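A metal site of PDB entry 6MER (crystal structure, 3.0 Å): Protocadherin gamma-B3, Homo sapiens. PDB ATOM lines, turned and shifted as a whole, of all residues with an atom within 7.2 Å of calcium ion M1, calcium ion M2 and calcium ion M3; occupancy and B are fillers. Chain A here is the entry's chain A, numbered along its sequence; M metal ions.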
ATOM      1  N   GLU A 114       0.784   3.490  -3.098  1.00  0.00           N
ATOM      2  CA  GLU A 114       0.783   3.912  -4.495  1.00  0.00           C
ATOM      3  C   GLU A 114       1.817   4.997  -4.775  1.00  0.00           C
ATOM      4  O   GLU A 114       2.232   5.145  -5.935  1.00  0.00           O
ATOM      5  CB  GLU A 114      -0.605   4.419  -4.887  1.00  0.00           C
ATOM      6  CG  GLU A 114      -1.743   3.467  -4.583  1.00  0.00           C
ATOM      7  CD  GLU A 114      -3.087   4.009  -5.018  1.00  0.00           C
ATOM      8  OE1 GLU A 114      -3.151   4.648  -6.090  1.00  0.00           O
ATOM      9  OE2 GLU A 114      -4.083   3.805  -4.299  1.00  0.00           O
ATOM     10  N   LEU A 170       2.657   2.079  -9.163  1.00  0.00           N
ATOM     11  CA  LEU A 170       1.592   1.234  -8.617  1.00  0.00           C
ATOM     12  C   LEU A 170       0.303   2.026  -8.513  1.00  0.00           C
ATOM     13  O   LEU A 170       0.282   3.126  -7.944  1.00  0.00           O
ATOM     14  CB  LEU A 170       1.986   0.690  -7.249  1.00  0.00           C
ATOM     15  CG  LEU A 170       3.107  -0.361  -7.216  1.00  0.00           C
ATOM     16  CD1 LEU A 170       3.321  -0.877  -5.809  1.00  0.00           C
ATOM     17  CD2 LEU A 170       2.793  -1.502  -8.179  1.00  0.00           C
ATOM     18  N   ASP A 171      -0.774   1.474  -9.059  1.00  0.00           N
ATOM     19  CA  ASP A 171      -2.103   2.069  -9.001  1.00  0.00           C
ATOM     20  C   ASP A 171      -3.046   1.043  -8.382  1.00  0.00           C
ATOM     21  O   ASP A 171      -3.396   0.057  -9.043  1.00  0.00           O
ATOM     22  CB  ASP A 171      -2.573   2.505 -10.384  1.00  0.00           C
ATOM     23  CG  ASP A 171      -3.865   3.310 -10.343  1.00  0.00           C
ATOM     24  OD1 ASP A 171      -4.372   3.565  -9.234  1.00  0.00           O
ATOM     25  OD2 ASP A 171      -4.357   3.690 -11.421  1.00  0.00           O
ATOM     26  N   ARG A 172      -3.439   1.260  -7.137  1.00  0.00           N
ATOM     27  CA  ARG A 172      -4.344   0.332  -6.470  1.00  0.00           C
ATOM     28  C   ARG A 172      -5.702   0.292  -7.156  1.00  0.00           C
ATOM     29  O   ARG A 172      -6.350  -0.765  -7.190  1.00  0.00           O
ATOM     30  CB  ARG A 172      -4.512   0.711  -5.002  1.00  0.00           C
ATOM     31  CG  ARG A 172      -5.290  -0.309  -4.174  1.00  0.00           C
ATOM     32  CD  ARG A 172      -5.908   0.334  -2.948  1.00  0.00           C
ATOM     33  NE  ARG A 172      -6.945   1.305  -3.306  1.00  0.00           N
ATOM     34  CZ  ARG A 172      -8.227   1.004  -3.456  1.00  0.00           C
ATOM     35  NH1 ARG A 172      -8.642  -0.240  -3.283  1.00  0.00           N
ATOM     36  NH2 ARG A 172      -9.101   1.947  -3.786  1.00  0.00           N
ATOM     37  N   GLU A 173      -6.142   1.420  -7.712  1.00  0.00           N
ATOM     38  CA  GLU A 173      -7.417   1.459  -8.432  1.00  0.00           C
ATOM     39  C   GLU A 173      -7.388   0.658  -9.724  1.00  0.00           C
ATOM     40  O   GLU A 173      -8.448   0.398 -10.292  1.00  0.00           O
ATOM     41  CB  GLU A 173      -7.804   2.909  -8.725  1.00  0.00           C
ATOM     42  CG  GLU A 173      -8.245   3.709  -7.503  1.00  0.00           C
ATOM     43  CD  GLU A 173      -7.112   4.008  -6.540  1.00  0.00           C
ATOM     44  OE1 GLU A 173      -5.985   4.283  -7.004  1.00  0.00           O
ATOM     45  OE2 GLU A 173      -7.339   3.960  -5.309  1.00  0.00           O
ATOM     46  N   GLU A 174      -6.204   0.274 -10.195  1.00  0.00           N
ATOM     47  CA  GLU A 174      -6.059  -0.593 -11.364  1.00  0.00           C
ATOM     48  C   GLU A 174      -5.745  -2.030 -10.999  1.00  0.00           C
ATOM     49  O   GLU A 174      -6.264  -2.958 -11.638  1.00  0.00           O
ATOM     50  CB  GLU A 174      -4.969  -0.040 -12.287  1.00  0.00           C
ATOM     51  CG  GLU A 174      -4.719  -0.863 -13.543  1.00  0.00           C
ATOM     52  CD  GLU A 174      -5.866  -0.783 -14.537  1.00  0.00           C
ATOM     53  OE1 GLU A 174      -6.663   0.187 -14.459  1.00  0.00           O
ATOM     54  OE2 GLU A 174      -5.978  -1.678 -15.390  1.00  0.00           O
ATOM     55  N   ALA A 203      -0.901  -0.637  -1.002  1.00  0.00           N
ATOM     56  CA  ALA A 203      -1.594   0.166  -0.011  1.00  0.00           C
ATOM     57  C   ALA A 203      -2.213   1.398  -0.666  1.00  0.00           C
ATOM     58  O   ALA A 203      -1.638   1.985  -1.587  1.00  0.00           O
ATOM     59  CB  ALA A 203      -0.642   0.587   1.103  1.00  0.00           C
ATOM     60  N   ASP A 204      -3.390   1.783  -0.189  1.00  0.00           N
ATOM     61  CA  ASP A 204      -4.118   2.890  -0.786  1.00  0.00           C
ATOM     62  C   ASP A 204      -3.471   4.225  -0.418  1.00  0.00           C
ATOM     63  O   ASP A 204      -2.961   4.405   0.688  1.00  0.00           O
ATOM     64  CB  ASP A 204      -5.582   2.886  -0.339  1.00  0.00           C
ATOM     65  CG  ASP A 204      -6.384   4.006  -0.959  1.00  0.00           C
ATOM     66  OD1 ASP A 204      -6.622   3.964  -2.181  1.00  0.00           O
ATOM     67  OD2 ASP A 204      -6.768   4.937  -0.222  1.00  0.00           O
ATOM     68  N   ALA A 205      -3.494   5.161  -1.368  1.00  0.00           N
ATOM     69  CA  ALA A 205      -3.010   6.514  -1.169  1.00  0.00           C
ATOM     70  C   ALA A 205      -4.049   7.492  -1.700  1.00  0.00           C
ATOM     71  O   ALA A 205      -4.624   7.271  -2.767  1.00  0.00           O
ATOM     72  CB  ALA A 205      -1.666   6.739  -1.856  1.00  0.00           C
ATOM     73  N   ASN A 206      -4.279   8.569  -0.952  1.00  0.00           N
ATOM     74  CA  ASN A 206      -5.287   9.562  -1.318  1.00  0.00           C
ATOM     75  C   ASN A 206      -4.770  10.383  -2.493  1.00  0.00           C
ATOM     76  O   ASN A 206      -4.244  11.494  -2.351  1.00  0.00           O
ATOM     77  CB  ASN A 206      -5.634  10.454  -0.129  1.00  0.00           C
ATOM     78  CG  ASN A 206      -6.738  11.435  -0.439  1.00  0.00           C
ATOM     79  OD1 ASN A 206      -6.488  12.592  -0.794  1.00  0.00           O
ATOM     80  ND2 ASN A 206      -7.984  10.991  -0.294  1.00  0.00           N
ATOM     81  N   ASP A 207      -4.937   9.821  -3.697  1.00  0.00           N
ATOM     82  CA  ASP A 207      -4.522  10.492  -4.928  1.00  0.00           C
ATOM     83  C   ASP A 207      -5.685  10.760  -5.870  1.00  0.00           C
ATOM     84  O   ASP A 207      -5.467  11.369  -6.930  1.00  0.00           O
ATOM     85  CB  ASP A 207      -3.446   9.668  -5.653  1.00  0.00           C
ATOM     86  CG  ASP A 207      -3.979   8.323  -6.142  1.00  0.00           C
ATOM     87  OD1 ASP A 207      -4.922   7.793  -5.526  1.00  0.00           O
ATOM     88  OD2 ASP A 207      -3.438   7.805  -7.138  1.00  0.00           O
ATOM     89  N   ASN A 208      -6.898  10.335  -5.530  1.00  0.00           N
ATOM     90  CA  ASN A 208      -8.072  10.573  -6.359  1.00  0.00           C
ATOM     91  C   ASN A 208      -9.033  11.499  -5.633  1.00  0.00           C
ATOM     92  O   ASN A 208      -9.723  11.075  -4.694  1.00  0.00           O
ATOM     93  CB  ASN A 208      -8.776   9.257  -6.708  1.00  0.00           C
ATOM     94  CG  ASN A 208      -7.950   8.388  -7.644  1.00  0.00           C
ATOM     95  OD1 ASN A 208      -6.724   8.517  -7.714  1.00  0.00           O
ATOM     96  ND2 ASN A 208      -8.615   7.496  -8.364  1.00  0.00           N
ATOM     97  N   PRO A 209      -9.112  12.778  -6.003  1.00  0.00           N
ATOM     98  CA  PRO A 209     -10.073  13.683  -5.368  1.00  0.00           C
ATOM     99  C   PRO A 209     -11.496  13.291  -5.696  1.00  0.00           C
ATOM    100  O   PRO A 209     -11.740  12.552  -6.667  1.00  0.00           O
ATOM    101  CB  PRO A 209      -9.717  15.061  -5.966  1.00  0.00           C
ATOM    102  CG  PRO A 209      -8.332  14.900  -6.512  1.00  0.00           C
ATOM    103  CD  PRO A 209      -8.246  13.470  -6.962  1.00  0.00           C
ATOM    104  N   PRO A 210     -12.479  13.755  -4.913  1.00  0.00           N
ATOM    105  CA  PRO A 210     -13.875  13.458  -5.242  1.00  0.00           C
ATOM    106  C   PRO A 210     -14.280  14.066  -6.574  1.00  0.00           C
ATOM    107  O   PRO A 210     -13.753  15.102  -6.991  1.00  0.00           O
ATOM    108  CB  PRO A 210     -14.650  14.085  -4.075  1.00  0.00           C
ATOM    109  CG  PRO A 210     -13.656  14.173  -2.955  1.00  0.00           C
ATOM    110  CD  PRO A 210     -12.342  14.447  -3.614  1.00  0.00           C
ATOM    111  N   ILE A 237     -18.043  10.611  -6.321  1.00  0.00           N
ATOM    112  CA  ILE A 237     -17.395   9.309  -6.432  1.00  0.00           C
ATOM    113  C   ILE A 237     -15.930   9.465  -6.052  1.00  0.00           C
ATOM    114  O   ILE A 237     -15.225  10.330  -6.592  1.00  0.00           O
ATOM    115  CB  ILE A 237     -17.540   8.740  -7.852  1.00  0.00           C
ATOM    116  CG1 ILE A 237     -19.009   8.460  -8.174  1.00  0.00           C
ATOM    117  CG2 ILE A 237     -16.711   7.472  -7.997  1.00  0.00           C
ATOM    118  CD1 ILE A 237     -19.646   7.445  -7.264  1.00  0.00           C
ATOM    119  N   ASP A 238     -15.479   8.631  -5.117  1.00  0.00           N
ATOM    120  CA  ASP A 238     -14.082   8.603  -4.688  1.00  0.00           C
ATOM    121  C   ASP A 238     -13.574   7.171  -4.860  1.00  0.00           C
ATOM    122  O   ASP A 238     -14.004   6.270  -4.142  1.00  0.00           O
ATOM    123  CB  ASP A 238     -13.949   9.064  -3.236  1.00  0.00           C
ATOM    124  CG  ASP A 238     -12.542   9.525  -2.900  1.00  0.00           C
ATOM    125  OD1 ASP A 238     -11.575   8.899  -3.383  1.00  0.00           O
ATOM    126  OD2 ASP A 238     -12.405  10.518  -2.156  1.00  0.00           O
ATOM    127  N   MET A 239     -12.664   6.983  -5.820  1.00  0.00           N
ATOM    128  CA  MET A 239     -12.184   5.650  -6.180  1.00  0.00           C
ATOM    129  C   MET A 239     -11.195   5.076  -5.182  1.00  0.00           C
ATOM    130  O   MET A 239     -10.729   3.950  -5.385  1.00  0.00           O
ATOM    131  CB  MET A 239     -11.543   5.699  -7.566  1.00  0.00           C
ATOM    132  CG  MET A 239     -12.482   6.145  -8.682  1.00  0.00           C
ATOM    133  SD  MET A 239     -13.866   5.019  -8.904  1.00  0.00           S
ATOM    134  CE  MET A 239     -13.011   3.501  -9.324  1.00  0.00           C
ATOM    135  N   ASP A 240     -10.868   5.795  -4.103  1.00  0.00           N
ATOM    136  CA  ASP A 240      -9.890   5.310  -3.137  1.00  0.00           C
ATOM    137  C   ASP A 240     -10.524   4.297  -2.184  1.00  0.00           C
ATOM    138  O   ASP A 240     -11.598   3.758  -2.452  1.00  0.00           O
ATOM    139  CB  ASP A 240      -9.278   6.475  -2.366  1.00  0.00           C
ATOM    140  CG  ASP A 240      -8.468   7.389  -3.247  1.00  0.00           C
ATOM    141  OD1 ASP A 240      -7.977   6.934  -4.304  1.00  0.00           O
ATOM    142  OD2 ASP A 240      -8.304   8.577  -2.886  1.00  0.00           O
ATOM    143  N   GLU A 241      -9.850   4.031  -1.061  1.00  0.00           N
ATOM    144  CA  GLU A 241     -10.268   2.997  -0.129  1.00  0.00           C
ATOM    145  C   GLU A 241     -10.240   3.538   1.296  1.00  0.00           C
ATOM    146  O   GLU A 241      -9.282   4.202   1.698  1.00  0.00           O
ATOM    147  CB  GLU A 241      -9.366   1.765  -0.228  1.00  0.00           C
ATOM    148  CG  GLU A 241      -9.641   0.690   0.806  1.00  0.00           C
ATOM    149  CD  GLU A 241      -8.635  -0.437   0.770  1.00  0.00           C
ATOM    150  OE1 GLU A 241      -7.766  -0.428  -0.126  1.00  0.00           O
ATOM    151  OE2 GLU A 241      -8.696  -1.321   1.656  1.00  0.00           O
ATOM    152  N   ILE A 243     -10.655   5.631   4.547  1.00  0.00           N
ATOM    153  CA  ILE A 243     -10.802   7.042   4.901  1.00  0.00           C
ATOM    154  C   ILE A 243     -10.598   7.932   3.683  1.00  0.00           C
ATOM    155  O   ILE A 243     -11.208   9.014   3.595  1.00  0.00           O
ATOM    156  CB  ILE A 243      -9.825   7.400   6.043  1.00  0.00           C
ATOM    157  CG1 ILE A 243      -9.938   8.870   6.425  1.00  0.00           C
ATOM    158  CG2 ILE A 243      -8.392   7.049   5.644  1.00  0.00           C
ATOM    159  CD1 ILE A 243     -11.314   9.272   6.920  1.00  0.00           C
ATOM    160  N   ASN A 244      -9.783   7.497   2.720  1.00  0.00           N
ATOM    161  CA  ASN A 244      -9.546   8.277   1.514  1.00  0.00           C
ATOM    162  C   ASN A 244     -10.729   8.251   0.550  1.00  0.00           C
ATOM    163  O   ASN A 244     -10.633   8.837  -0.533  1.00  0.00           O
ATOM    164  CB  ASN A 244      -8.288   7.775   0.815  1.00  0.00           C
ATOM    165  CG  ASN A 244      -7.071   7.796   1.707  1.00  0.00           C
ATOM    166  OD1 ASN A 244      -6.974   8.618   2.622  1.00  0.00           O
ATOM    167  ND2 ASN A 244      -6.122   6.907   1.447  1.00  0.00           N
ATOM    168  N   ALA A 245     -11.835   7.588   0.911  1.00  0.00           N
ATOM    169  CA  ALA A 245     -13.016   7.544   0.074  1.00  0.00           C
ATOM    170  C   ALA A 245     -14.277   8.070   0.756  1.00  0.00           C
ATOM    171  O   ALA A 245     -15.281   8.287   0.072  1.00  0.00           O
ATOM    172  CB  ALA A 245     -13.273   6.119  -0.419  1.00  0.00           C
ATOM    173  N   GLU A 246     -14.255   8.256   2.073  1.00  0.00           N
ATOM    174  CA  GLU A 246     -15.410   8.788   2.785  1.00  0.00           C
ATOM    175  C   GLU A 246     -15.552  10.281   2.470  1.00  0.00           C
ATOM    176  O   GLU A 246     -14.615  11.048   2.677  1.00  0.00           O
ATOM    177  CB  GLU A 246     -15.268   8.563   4.277  1.00  0.00           C
ATOM    178  CG  GLU A 246     -15.172   7.090   4.674  1.00  0.00           C
ATOM    179  CD  GLU A 246     -14.923   6.902   6.158  1.00  0.00           C
ATOM    180  OE1 GLU A 246     -14.721   7.914   6.867  1.00  0.00           O
ATOM    181  OE2 GLU A 246     -14.930   5.737   6.613  1.00  0.00           O
ATOM    182  N   ILE A 247     -16.726  10.666   1.980  1.00  0.00           N
ATOM    183  CA  ILE A 247     -16.975  12.021   1.504  1.00  0.00           C
ATOM    184  C   ILE A 247     -17.979  12.707   2.417  1.00  0.00           C
ATOM    185  O   ILE A 247     -18.974  12.102   2.823  1.00  0.00           O
ATOM    186  CB  ILE A 247     -17.482  12.009   0.051  1.00  0.00           C
ATOM    187  CG1 ILE A 247     -16.560  11.159  -0.830  1.00  0.00           C
ATOM    188  CG2 ILE A 247     -17.587  13.429  -0.501  1.00  0.00           C
ATOM    189  CD1 ILE A 247     -17.075  10.947  -2.225  1.00  0.00           C
ATOM    190  N   ASP A 293     -12.760  14.746   1.552  1.00  0.00           N
ATOM    191  CA  ASP A 293     -12.478  13.408   2.048  1.00  0.00           C
ATOM    192  C   ASP A 293     -11.484  13.485   3.216  1.00  0.00           C
ATOM    193  O   ASP A 293     -11.200  14.565   3.751  1.00  0.00           O
ATOM    194  CB  ASP A 293     -11.962  12.502   0.926  1.00  0.00           C
ATOM    195  CG  ASP A 293     -10.722  13.069   0.245  1.00  0.00           C
ATOM    196  OD1 ASP A 293     -10.347  14.222   0.547  1.00  0.00           O
ATOM    197  OD2 ASP A 293     -10.125  12.347  -0.579  1.00  0.00           O
ATOM    198  N   GLY A 294     -10.949  12.322   3.599  1.00  0.00           N
ATOM    199  CA  GLY A 294      -9.981  12.282   4.677  1.00  0.00           C
ATOM    200  C   GLY A 294      -8.653  12.932   4.318  1.00  0.00           C
ATOM    201  O   GLY A 294      -7.980  13.492   5.179  1.00  0.00           O
ATOM    202  N   GLY A 295      -8.265  12.851   3.039  1.00  0.00           N
ATOM    203  CA  GLY A 295      -7.042  13.451   2.563  1.00  0.00           C
ATOM    204  C   GLY A 295      -7.130  14.925   2.266  1.00  0.00           C
ATOM    205  O   GLY A 295      -6.211  15.480   1.644  1.00  0.00           O
ATOM    206  N   HIS A 297      -8.767  16.481   0.120  1.00  0.00           N
ATOM    207  CA  HIS A 297      -8.976  16.812  -1.277  1.00  0.00           C
ATOM    208  C   HIS A 297     -10.400  17.338  -1.472  1.00  0.00           C
ATOM    209  O   HIS A 297     -11.370  16.674  -1.103  1.00  0.00           O
ATOM    210  CB  HIS A 297      -8.729  15.591  -2.163  1.00  0.00           C
ATOM    211  CG  HIS A 297      -7.293  15.409  -2.547  1.00  0.00           C
ATOM    212  ND1 HIS A 297      -6.883  14.450  -3.452  1.00  0.00           N
ATOM    213  CD2 HIS A 297      -6.181  16.061  -2.154  1.00  0.00           C
ATOM    214  CE1 HIS A 297      -5.574  14.516  -3.596  1.00  0.00           C
ATOM    215  NE2 HIS A 297      -5.120  15.488  -2.823  1.00  0.00           N
HETATM  216 CA    CA M   1      -9.789  10.438  -2.280  1.00  0.00          CA
HETATM  217 CA    CA M   2      -5.783   5.582  -4.194  1.00  0.00          CA
HETATM  218 CA    CA M   3      -4.220   5.686  -8.081  1.00  0.00          CA
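Calcium ion M2 is bound by OE2 of Glu 114 (2.5 Å).
O of Ala 205 binds calcium ion M2.
Calcium ion M2 is bound by the side-chain carboxylate (OE2) of Glu 173 (2.5 Å).
OD1 of Asp 240 is bound to calcium ion M2 (2.6 Å).
The side-chain carboxylate (OD1) of Asp 204 binds calcium ion M2, 2.7 Å away.
OD1 of Asp 207 is bound to calcium ion M2 (2.7 Å).
Slightly farther from calcium ion M2 lies OE1 of Glu 173 (3.1 Å).
OD1 of Asp 207 sits close to OD1 of Asn 208, 2.9 Å away.
The backbone carbonyl oxygen (O) of Asp 240 sits close to the guanidinium group (NH2) of Arg 172, 3.4 Å away.
OE2 of Glu 114 sits close to NE of Arg 172, at 3.9 Å.
The backbone NH of Glu 114 sits at hydrogen-bond distance from the backbone carbonyl oxygen of Ala 203 (3.2 Å).
The side-chain carboxylate (OE2) of Glu 173 sits close to the guanidinium group (NH2) of Arg 172 (3.1 Å).
ND2 of Asn 244 sits at hydrogen-bond distance from OD2 of Asp 204, at 2.7 Å.
OD1 of Asp 204 sits close to NE of Arg 172 (2.9 Å).
The side-chain amide oxygen of Asn 206 sits at hydrogen-bond distance from a ring nitrogen (ND1) of His 297 (3.3 Å).
Within 4 Å of calcium ion M2: Glu 114, Glu 173, Asp 204, Ala 205, Asp 207 and Asp 240.
Along chain A the residues within 4 Å of calcium ion M2 span positions 114 to 240.
The nearest printed residue that does not touch calcium ion M2 is Arg 172 (4.5 Å).
OD1 of Asp 171 is bound to calcium ion M3.
OD2 of Asp 207 is bound to calcium ion M3, 2.4 Å away.
OE1 of Glu 114 binds calcium ion M3 (2.5 Å).
OE1 of Glu 173 binds calcium ion M3, at 2.5 Å.
Calcium ion M3 has four donor atoms within binding distance.
Five residues have an atom within 4 Å of calcium ion M3: Glu 114, Asp 171, Glu 173, Asp 207 and Asn 208.
The nearest printed residue that does not touch calcium ion M3 is Arg 172 (4.6 Å).
OD2 of Asp 240 is bound to calcium ion M1, 2.5 Å away.
Calcium ion M1 is bound by O of Asn 208.
O of Asn 244 binds calcium ion M1, 2.5 Å away.
Calcium ion M1 is bound by the side-chain carboxylate (OD2) of Asp 293 (2.6 Å).
OD1 of Asp 238 binds calcium ion M1, at 2.6 Å.
Calcium ion M1 is bound by OD2 of Asp 238 (2.6 Å).
Calcium ion M1 is bound by the side-chain amide nitrogen (ND2) of Asn 206, at 2.7 Å.
Within 4 Å of calcium ion M1: Asn 206, Asn 208, Asp 238, Asp 240, Asn 244 and Asp 293.
Along chain A the residues within 4 Å of calcium ion M1 span positions 206 to 293.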
